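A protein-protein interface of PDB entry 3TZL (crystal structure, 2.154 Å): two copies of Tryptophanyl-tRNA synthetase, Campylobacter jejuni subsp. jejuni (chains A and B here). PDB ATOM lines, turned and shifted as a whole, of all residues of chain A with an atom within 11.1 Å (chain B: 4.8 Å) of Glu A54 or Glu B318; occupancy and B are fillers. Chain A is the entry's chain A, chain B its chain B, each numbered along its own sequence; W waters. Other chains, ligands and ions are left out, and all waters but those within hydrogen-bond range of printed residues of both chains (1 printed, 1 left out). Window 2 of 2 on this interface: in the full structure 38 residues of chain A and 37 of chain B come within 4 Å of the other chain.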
ATOM      1  N   PRO A  12     -36.864  32.228  -4.163  1.00  0.00           N
ATOM      2  CA  PRO A  12     -35.454  32.633  -4.070  1.00  0.00           C
ATOM      3  C   PRO A  12     -34.896  33.157  -5.400  1.00  0.00           C
ATOM      4  O   PRO A  12     -33.776  33.679  -5.430  1.00  0.00           O
ATOM      5  CB  PRO A  12     -34.744  31.339  -3.673  1.00  0.00           C
ATOM      6  CG  PRO A  12     -35.629  30.266  -4.224  1.00  0.00           C
ATOM      7  CD  PRO A  12     -37.027  30.767  -4.064  1.00  0.00           C
ATOM      8  N   ASN A  43     -37.224  26.748  -2.134  1.00  0.00           N
ATOM      9  CA  ASN A  43     -36.212  26.265  -3.070  1.00  0.00           C
ATOM     10  C   ASN A  43     -36.544  24.976  -3.840  1.00  0.00           C
ATOM     11  O   ASN A  43     -35.941  24.721  -4.885  1.00  0.00           O
ATOM     12  CB  ASN A  43     -34.842  26.145  -2.402  1.00  0.00           C
ATOM     13  CG  ASN A  43     -34.834  25.145  -1.273  1.00  0.00           C
ATOM     14  OD1 ASN A  43     -35.811  25.025  -0.532  1.00  0.00           O
ATOM     15  ND2 ASN A  43     -33.725  24.423  -1.127  1.00  0.00           N
ATOM     16  N   ALA A  46     -38.197  26.464  -6.818  1.00  0.00           N
ATOM     17  CA  ALA A  46     -37.212  27.096  -7.694  1.00  0.00           C
ATOM     18  C   ALA A  46     -36.615  26.122  -8.682  1.00  0.00           C
ATOM     19  O   ALA A  46     -36.142  26.537  -9.732  1.00  0.00           O
ATOM     20  CB  ALA A  46     -36.110  27.751  -6.884  1.00  0.00           C
ATOM     21  N   MET A  47     -36.649  24.829  -8.371  1.00  0.00           N
ATOM     22  CA  MET A  47     -36.116  23.814  -9.292  1.00  0.00           C
ATOM     23  C   MET A  47     -36.977  23.607 -10.528  1.00  0.00           C
ATOM     24  O   MET A  47     -36.571  22.901 -11.464  1.00  0.00           O
ATOM     25  CB  MET A  47     -35.988  22.460  -8.583  1.00  0.00           C
ATOM     26  CG  MET A  47     -35.048  22.443  -7.410  1.00  0.00           C
ATOM     27  SD  MET A  47     -35.195  20.833  -6.298  1.00  0.00           S
ATOM     28  CE  MET A  47     -33.900  21.366  -4.955  1.00  0.00           C
ATOM     29  N   SER A  50     -35.097  26.025 -13.121  1.00  0.00           N
ATOM     30  CA  SER A  50     -33.662  25.852 -13.340  1.00  0.00           C
ATOM     31  C   SER A  50     -33.136  24.618 -12.587  1.00  0.00           C
ATOM     32  O   SER A  50     -33.585  24.323 -11.481  1.00  0.00           O
ATOM     33  CB  SER A  50     -32.907  27.121 -12.890  1.00  0.00           C
ATOM     34  OG  SER A  50     -31.508  26.899 -12.756  1.00  0.00           O
ATOM     35  N   GLN A  51     -32.183  23.915 -13.193  1.00  0.00           N
ATOM     36  CA  GLN A  51     -31.466  22.825 -12.541  1.00  0.00           C
ATOM     37  C   GLN A  51     -29.959  23.128 -12.479  1.00  0.00           C
ATOM     38  O   GLN A  51     -29.137  22.214 -12.428  1.00  0.00           O
ATOM     39  CB  GLN A  51     -31.738  21.489 -13.257  1.00  0.00           C
ATOM     40  CG  GLN A  51     -33.229  21.098 -13.290  1.00  0.00           C
ATOM     41  CD  GLN A  51     -34.016  21.850 -14.370  1.00  0.00           C
ATOM     42  OE1 GLN A  51     -33.660  21.811 -15.548  1.00  0.00           O
ATOM     43  NE2 GLN A  51     -35.086  22.535 -13.969  1.00  0.00           N
ATOM     44  N   ASP A  52     -29.606  24.413 -12.483  1.00  0.00           N
ATOM     45  CA  ASP A  52     -28.218  24.828 -12.276  1.00  0.00           C
ATOM     46  C   ASP A  52     -28.005  24.951 -10.778  1.00  0.00           C
ATOM     47  O   ASP A  52     -28.300  25.990 -10.183  1.00  0.00           O
ATOM     48  CB  ASP A  52     -27.948  26.170 -12.967  1.00  0.00           C
ATOM     49  CG  ASP A  52     -26.547  26.712 -12.702  1.00  0.00           C
ATOM     50  OD1 ASP A  52     -25.805  26.149 -11.877  1.00  0.00           O
ATOM     51  OD2 ASP A  52     -26.181  27.736 -13.321  1.00  0.00           O
ATOM     52  N   GLY A  53     -27.472  23.892 -10.174  1.00  0.00           N
ATOM     53  CA  GLY A  53     -27.429  23.768  -8.725  1.00  0.00           C
ATOM     54  C   GLY A  53     -26.565  24.791  -8.017  1.00  0.00           C
ATOM     55  O   GLY A  53     -26.858  25.200  -6.900  1.00  0.00           O
ATOM     56  N   GLU A  54     -25.490  25.207  -8.667  1.00  0.00           N
ATOM     57  CA  GLU A  54     -24.575  26.151  -8.057  1.00  0.00           C
ATOM     58  C   GLU A  54     -25.283  27.504  -7.905  1.00  0.00           C
ATOM     59  O   GLU A  54     -25.185  28.161  -6.879  1.00  0.00           O
ATOM     60  CB  GLU A  54     -23.286  26.258  -8.891  1.00  0.00           C
ATOM     61  CG  GLU A  54     -22.645  24.881  -9.259  1.00  0.00           C
ATOM     62  CD  GLU A  54     -23.396  24.082 -10.355  1.00  0.00           C
ATOM     63  OE1 GLU A  54     -23.714  24.655 -11.418  1.00  0.00           O
ATOM     64  OE2 GLU A  54     -23.657  22.872 -10.154  1.00  0.00           O
ATOM     65  N   LYS A  55     -26.038  27.878  -8.926  1.00  0.00           N
ATOM     66  CA  LYS A  55     -26.816  29.096  -8.920  1.00  0.00           C
ATOM     67  C   LYS A  55     -27.991  29.002  -7.943  1.00  0.00           C
ATOM     68  O   LYS A  55     -28.222  29.942  -7.160  1.00  0.00           O
ATOM     69  CB  LYS A  55     -27.320  29.382 -10.332  1.00  0.00           C
ATOM     70  CG  LYS A  55     -28.147  30.631 -10.463  1.00  0.00           C
ATOM     71  CD  LYS A  55     -28.250  31.066 -11.921  1.00  0.00           C
ATOM     72  CE  LYS A  55     -26.891  31.506 -12.487  1.00  0.00           C
ATOM     73  NZ  LYS A  55     -27.017  32.318 -13.748  1.00  0.00           N
ATOM     74  N   LEU A  56     -28.728  27.885  -7.993  1.00  0.00           N
ATOM     75  CA  LEU A  56     -29.899  27.674  -7.119  1.00  0.00           C
ATOM     76  C   LEU A  56     -29.487  27.775  -5.663  1.00  0.00           C
ATOM     77  O   LEU A  56     -30.184  28.375  -4.835  1.00  0.00           O
ATOM     78  CB  LEU A  56     -30.579  26.303  -7.370  1.00  0.00           C
ATOM     79  CG  LEU A  56     -31.336  26.068  -8.682  1.00  0.00           C
ATOM     80  CD1 LEU A  56     -31.832  24.613  -8.807  1.00  0.00           C
ATOM     81  CD2 LEU A  56     -32.498  27.047  -8.815  1.00  0.00           C
ATOM     82  N   LYS A  57     -28.336  27.192  -5.358  1.00  0.00           N
ATOM     83  CA  LYS A  57     -27.822  27.173  -3.994  1.00  0.00           C
ATOM     84  C   LYS A  57     -27.463  28.561  -3.484  1.00  0.00           C
ATOM     85  O   LYS A  57     -27.716  28.880  -2.321  1.00  0.00           O
ATOM     86  CB  LYS A  57     -26.596  26.267  -3.915  1.00  0.00           C
ATOM     87  CG  LYS A  57     -26.091  26.054  -2.493  1.00  0.00           C
ATOM     88  CD  LYS A  57     -24.969  25.034  -2.460  1.00  0.00           C
ATOM     89  CE  LYS A  57     -24.868  24.358  -1.076  1.00  0.00           C
ATOM     90  NZ  LYS A  57     -23.649  23.515  -0.900  1.00  0.00           N
ATOM     91  N   GLN A  58     -26.855  29.378  -4.342  1.00  0.00           N
ATOM     92  CA  GLN A  58     -26.531  30.757  -3.989  1.00  0.00           C
ATOM     93  C   GLN A  58     -27.770  31.619  -3.919  1.00  0.00           C
ATOM     94  O   GLN A  58     -27.855  32.503  -3.094  1.00  0.00           O
ATOM     95  CB  GLN A  58     -25.551  31.373  -4.991  1.00  0.00           C
ATOM     96  CG  GLN A  58     -24.136  30.925  -4.764  1.00  0.00           C
ATOM     97  CD  GLN A  58     -23.754  31.027  -3.298  1.00  0.00           C
ATOM     98  OE1 GLN A  58     -23.710  32.125  -2.743  1.00  0.00           O
ATOM     99  NE2 GLN A  58     -23.500  29.879  -2.658  1.00  0.00           N
ATOM    100  N   ASN A  59     -28.721  31.367  -4.808  1.00  0.00           N
ATOM    101  CA  ASN A  59     -29.980  32.090  -4.772  1.00  0.00           C
ATOM    102  C   ASN A  59     -30.667  31.874  -3.423  1.00  0.00           C
ATOM    103  O   ASN A  59     -31.242  32.804  -2.860  1.00  0.00           O
ATOM    104  CB  ASN A  59     -30.902  31.661  -5.919  1.00  0.00           C
ATOM    105  CG  ASN A  59     -30.482  32.236  -7.260  1.00  0.00           C
ATOM    106  OD1 ASN A  59     -29.462  32.924  -7.373  1.00  0.00           O
ATOM    107  ND2 ASN A  59     -31.276  31.962  -8.286  1.00  0.00           N
ATOM    108  N   SER A  60     -30.583  30.656  -2.888  1.00  0.00           N
ATOM    109  CA  SER A  60     -31.214  30.371  -1.602  1.00  0.00           C
ATOM    110  C   SER A  60     -30.520  31.088  -0.449  1.00  0.00           C
ATOM    111  O   SER A  60     -31.184  31.630   0.431  1.00  0.00           O
ATOM    112  CB  SER A  60     -31.296  28.868  -1.323  1.00  0.00           C
ATOM    113  OG  SER A  60     -32.207  28.251  -2.227  1.00  0.00           O
ATOM    114  N   LEU A  61     -29.193  31.078  -0.449  1.00  0.00           N
ATOM    115  CA  LEU A  61     -28.444  31.781   0.584  1.00  0.00           C
ATOM    116  C   LEU A  61     -28.761  33.260   0.537  1.00  0.00           C
ATOM    117  O   LEU A  61     -29.034  33.865   1.562  1.00  0.00           O
ATOM    118  CB  LEU A  61     -26.942  31.583   0.400  1.00  0.00           C
ATOM    119  CG  LEU A  61     -26.395  30.240   0.863  1.00  0.00           C
ATOM    120  CD1 LEU A  61     -24.891  30.170   0.607  1.00  0.00           C
ATOM    121  CD2 LEU A  61     -26.697  30.049   2.344  1.00  0.00           C
ATOM    122  N   LYS A  62     -28.726  33.840  -0.660  1.00  0.00           N
ATOM    123  CA  LYS A  62     -28.955  35.269  -0.815  1.00  0.00           C
ATOM    124  C   LYS A  62     -30.351  35.676  -0.353  1.00  0.00           C
ATOM    125  O   LYS A  62     -30.510  36.682   0.340  1.00  0.00           O
ATOM    126  CB  LYS A  62     -28.691  35.721  -2.253  1.00  0.00           C
ATOM    127  CG  LYS A  62     -27.206  35.807  -2.568  1.00  0.00           C
ATOM    128  CD  LYS A  62     -26.938  36.429  -3.923  1.00  0.00           C
ATOM    129  CE  LYS A  62     -27.241  35.466  -5.063  1.00  0.00           C
ATOM    130  NZ  LYS A  62     -26.640  35.933  -6.361  1.00  0.00           N
ATOM    131  N   ALA A  63     -31.357  34.884  -0.714  1.00  0.00           N
ATOM    132  CA  ALA A  63     -32.729  35.164  -0.295  1.00  0.00           C
ATOM    133  C   ALA A  63     -32.872  35.122   1.231  1.00  0.00           C
ATOM    134  O   ALA A  63     -33.510  35.998   1.823  1.00  0.00           O
ATOM    135  CB  ALA A  63     -33.706  34.201  -0.968  1.00  0.00           C
ATOM    136  N   LYS A  86     -38.310  17.910   5.092  1.00  0.00           N
ATOM    137  CA  LYS A  86     -38.549  17.000   3.970  1.00  0.00           C
ATOM    138  C   LYS A  86     -39.923  16.320   3.980  1.00  0.00           C
ATOM    139  O   LYS A  86     -40.326  15.682   2.996  1.00  0.00           O
ATOM    140  CB  LYS A  86     -37.403  15.999   3.876  1.00  0.00           C
ATOM    141  CG  LYS A  86     -36.119  16.704   3.403  1.00  0.00           C
ATOM    142  CD  LYS A  86     -34.914  15.796   3.304  1.00  0.00           C
ATOM    143  CE  LYS A  86     -33.630  16.629   3.171  1.00  0.00           C
ATOM    144  NZ  LYS A  86     -33.576  17.519   1.958  1.00  0.00           N
ATOM    145  N   GLN B 314     -26.199  12.224  -2.329  1.00  0.00           N
ATOM    146  CA  GLN B 314     -25.057  13.120  -2.110  1.00  0.00           C
ATOM    147  C   GLN B 314     -24.570  13.680  -3.449  1.00  0.00           C
ATOM    148  O   GLN B 314     -24.215  14.858  -3.554  1.00  0.00           O
ATOM    149  CB  GLN B 314     -23.912  12.386  -1.394  1.00  0.00           C
ATOM    150  CG  GLN B 314     -24.119  12.228   0.110  1.00  0.00           C
ATOM    151  CD  GLN B 314     -23.195  11.187   0.769  1.00  0.00           C
ATOM    152  OE1 GLN B 314     -22.150  10.803   0.226  1.00  0.00           O
ATOM    153  NE2 GLN B 314     -23.601  10.718   1.948  1.00  0.00           N
ATOM    154  N   LYS B 315     -24.560  12.825  -4.469  1.00  0.00           N
ATOM    155  CA  LYS B 315     -24.196  13.246  -5.815  1.00  0.00           C
ATOM    156  C   LYS B 315     -25.255  14.165  -6.409  1.00  0.00           C
ATOM    157  O   LYS B 315     -24.932  15.196  -7.007  1.00  0.00           O
ATOM    158  CB  LYS B 315     -24.000  12.028  -6.719  1.00  0.00           C
ATOM    159  CG  LYS B 315     -22.802  11.184  -6.332  1.00  0.00           C
ATOM    160  CD  LYS B 315     -22.688   9.982  -7.260  1.00  0.00           C
ATOM    161  CE  LYS B 315     -21.482   9.113  -6.926  1.00  0.00           C
ATOM    162  NZ  LYS B 315     -21.416   7.932  -7.840  1.00  0.00           N
ATOM    163  N   ILE B 316     -26.518  13.783  -6.257  1.00  0.00           N
ATOM    164  CA  ILE B 316     -27.611  14.593  -6.765  1.00  0.00           C
ATOM    165  C   ILE B 316     -27.633  15.977  -6.121  1.00  0.00           C
ATOM    166  O   ILE B 316     -27.868  16.977  -6.798  1.00  0.00           O
ATOM    167  CB  ILE B 316     -28.957  13.928  -6.514  1.00  0.00           C
ATOM    168  CG1 ILE B 316     -29.014  12.569  -7.229  1.00  0.00           C
ATOM    169  CG2 ILE B 316     -30.097  14.864  -6.924  1.00  0.00           C
ATOM    170  CD1 ILE B 316     -29.070  12.670  -8.689  1.00  0.00           C
ATOM    171  N   TYR B 317     -27.393  16.019  -4.813  1.00  0.00           N
ATOM    172  CA  TYR B 317     -27.392  17.271  -4.061  1.00  0.00           C
ATOM    173  C   TYR B 317     -26.370  18.259  -4.595  1.00  0.00           C
ATOM    174  O   TYR B 317     -26.628  19.468  -4.644  1.00  0.00           O
ATOM    175  CB  TYR B 317     -27.067  17.026  -2.586  1.00  0.00           C
ATOM    176  CG  TYR B 317     -28.265  16.659  -1.732  1.00  0.00           C
ATOM    177  CD1 TYR B 317     -29.437  16.207  -2.310  1.00  0.00           C
ATOM    178  CD2 TYR B 317     -28.223  16.795  -0.337  1.00  0.00           C
ATOM    179  CE1 TYR B 317     -30.542  15.878  -1.529  1.00  0.00           C
ATOM    180  CE2 TYR B 317     -29.324  16.469   0.458  1.00  0.00           C
ATOM    181  CZ  TYR B 317     -30.477  16.001  -0.151  1.00  0.00           C
ATOM    182  OH  TYR B 317     -31.578  15.662   0.604  1.00  0.00           O
ATOM    183  N   GLU B 318     -25.202  17.750  -4.968  1.00  0.00           N
ATOM    184  CA  GLU B 318     -24.167  18.608  -5.528  1.00  0.00           C
ATOM    185  C   GLU B 318     -24.649  19.255  -6.834  1.00  0.00           C
ATOM    186  O   GLU B 318     -24.311  20.412  -7.120  1.00  0.00           O
ATOM    187  CB  GLU B 318     -22.861  17.847  -5.735  1.00  0.00           C
ATOM    188  CG  GLU B 318     -21.724  18.694  -6.322  1.00  0.00           C
ATOM    189  CD  GLU B 318     -21.105  19.694  -5.320  1.00  0.00           C
ATOM    190  OE1 GLU B 318     -21.686  19.921  -4.231  1.00  0.00           O
ATOM    191  OE2 GLU B 318     -20.028  20.254  -5.619  1.00  0.00           O
ATOM    192  N   LYS B 319     -25.469  18.530  -7.599  1.00  0.00           N
ATOM    193  CA  LYS B 319     -25.935  19.040  -8.894  1.00  0.00           C
ATOM    194  C   LYS B 319     -27.151  19.959  -8.807  1.00  0.00           C
ATOM    195  O   LYS B 319     -27.336  20.814  -9.672  1.00  0.00           O
ATOM    196  CB  LYS B 319     -26.222  17.891  -9.869  1.00  0.00           C
ATOM    197  CG  LYS B 319     -25.049  16.925 -10.062  1.00  0.00           C
ATOM    198  CD  LYS B 319     -23.776  17.669 -10.447  1.00  0.00           C
ATOM    199  CE  LYS B 319     -23.744  18.016 -11.909  1.00  0.00           C
ATOM    200  NZ  LYS B 319     -22.739  19.075 -12.208  1.00  0.00           N
ATOM    201  N   ILE B 320     -27.990  19.779  -7.783  1.00  0.00           N
ATOM    202  CA  ILE B 320     -29.244  20.539  -7.703  1.00  0.00           C
ATOM    203  C   ILE B 320     -29.139  21.669  -6.671  1.00  0.00           C
ATOM    204  O   ILE B 320     -30.022  22.529  -6.562  1.00  0.00           O
ATOM    205  CB  ILE B 320     -30.448  19.623  -7.372  1.00  0.00           C
ATOM    206  CG1 ILE B 320     -31.776  20.322  -7.698  1.00  0.00           C
ATOM    207  CG2 ILE B 320     -30.414  19.227  -5.916  1.00  0.00           C
ATOM    208  CD1 ILE B 320     -31.984  20.629  -9.186  1.00  0.00           C
ATOM    209  N   GLY B 321     -28.048  21.664  -5.915  1.00  0.00           N
ATOM    210  CA  GLY B 321     -27.742  22.768  -5.029  1.00  0.00           C
ATOM    211  C   GLY B 321     -28.208  22.590  -3.595  1.00  0.00           C
ATOM    212  O   GLY B 321     -28.380  23.574  -2.879  1.00  0.00           O
ATOM    213  N   LEU B 322     -28.411  21.347  -3.166  1.00  0.00           N
ATOM    214  CA  LEU B 322     -28.882  21.099  -1.810  1.00  0.00           C
ATOM    215  C   LEU B 322     -27.718  20.753  -0.905  1.00  0.00           C
ATOM    216  O   LEU B 322     -27.838  20.857   0.319  1.00  0.00           O
ATOM    217  CB  LEU B 322     -29.918  19.980  -1.777  1.00  0.00           C
ATOM    218  CG  LEU B 322     -31.263  20.357  -2.373  1.00  0.00           C
ATOM    219  CD1 LEU B 322     -32.224  19.193  -2.273  1.00  0.00           C
ATOM    220  CD2 LEU B 322     -31.794  21.605  -1.639  1.00  0.00           C
ATOM    221  OXT LEU B 322     -26.649  20.372  -1.389  1.00  0.00           O
HETATM  222  O   HOH W   1     -25.542  21.758 -11.701  1.00  0.00           O
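Of the 19 printed residues of chain A, 8 touch a printed residue of chain B. Hydrophobic or aromatic side chains of chain A within 4 Å of the printed part of chain B: Met A47 and Leu A56. Hydrophobic or aromatic side chains of chain B within 4 Å of the printed part of chain A: Tyr B317, Ile B320 and Leu B322. Among the printed residues, no Asp or Glu carboxylate lies within 4 Å of a Lys or Arg side-chain nitrogen of the other chain.
Among the printed residues, merely in contact across the chains: Asn A43 with Leu B322, Met A47 with Ile B320, Met A47 with Leu B322, Gln A51 with Lys B319, Gly A53 with Ile B320, Gly A53 with Gly B321, Glu A54 with Glu B318, Leu A56 with Ile B320 and Lys A57 with Gly B321.
No position is printed for both chains.
Water W1 lies within hydrogen-bond range of OE2 of Glu A54 (2.7 Å), O of Lys B319 (2.9 Å) and N of Gly A53 (3.3 Å).
Glu B318 touches just one residue of chain A: Glu A54. Of the printed residues of chain A, Ile B320 touches Met A47, Gly A53 and Leu A56. Of the printed residues of chain A, Tyr B317 touches Lys A86 (3.0 Å). Of the printed residues of chain B, Met A47 touches Ile B320 and Leu B322. Printed residues of chain B within 4 Å of Lys A57: Gly B321. Printed residues of chain B within 4 Å of Gln A51: Lys B319 (3.6 Å). Gln A58 touches none of the printed residues of chain B. Ile B316 touches none of the printed residues of chain A. The nearest residue of chain A that does not touch Glu B318 is Gly A53 (4.9 Å). The nearest printed residue of chain B that does not touch Lys A86 is Leu B322 (4.7 Å).
The side-chain amide nitrogen of Gln A51 is in hydrogen-bond range of the backbone carbonyl oxygen of Met A47. OD1 of Asp A52 lies close to N of Glu A54, at 3.4 Å. The backbone carbonyl oxygen (O) of Leu A56 lies within hydrogen-bond range of the side-chain hydroxyl (OG) of Ser A60, at 3.3 Å. The backbone carbonyl oxygen (O) of Tyr B317 is in hydrogen-bond range of the backbone NH (N) of Leu B322 (3.0 Å).
N of Gly A53 lies close to O of Lys B319. NZ of Lys A86 lies within hydrogen-bond range of OH of Tyr B317 (3.0 Å).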
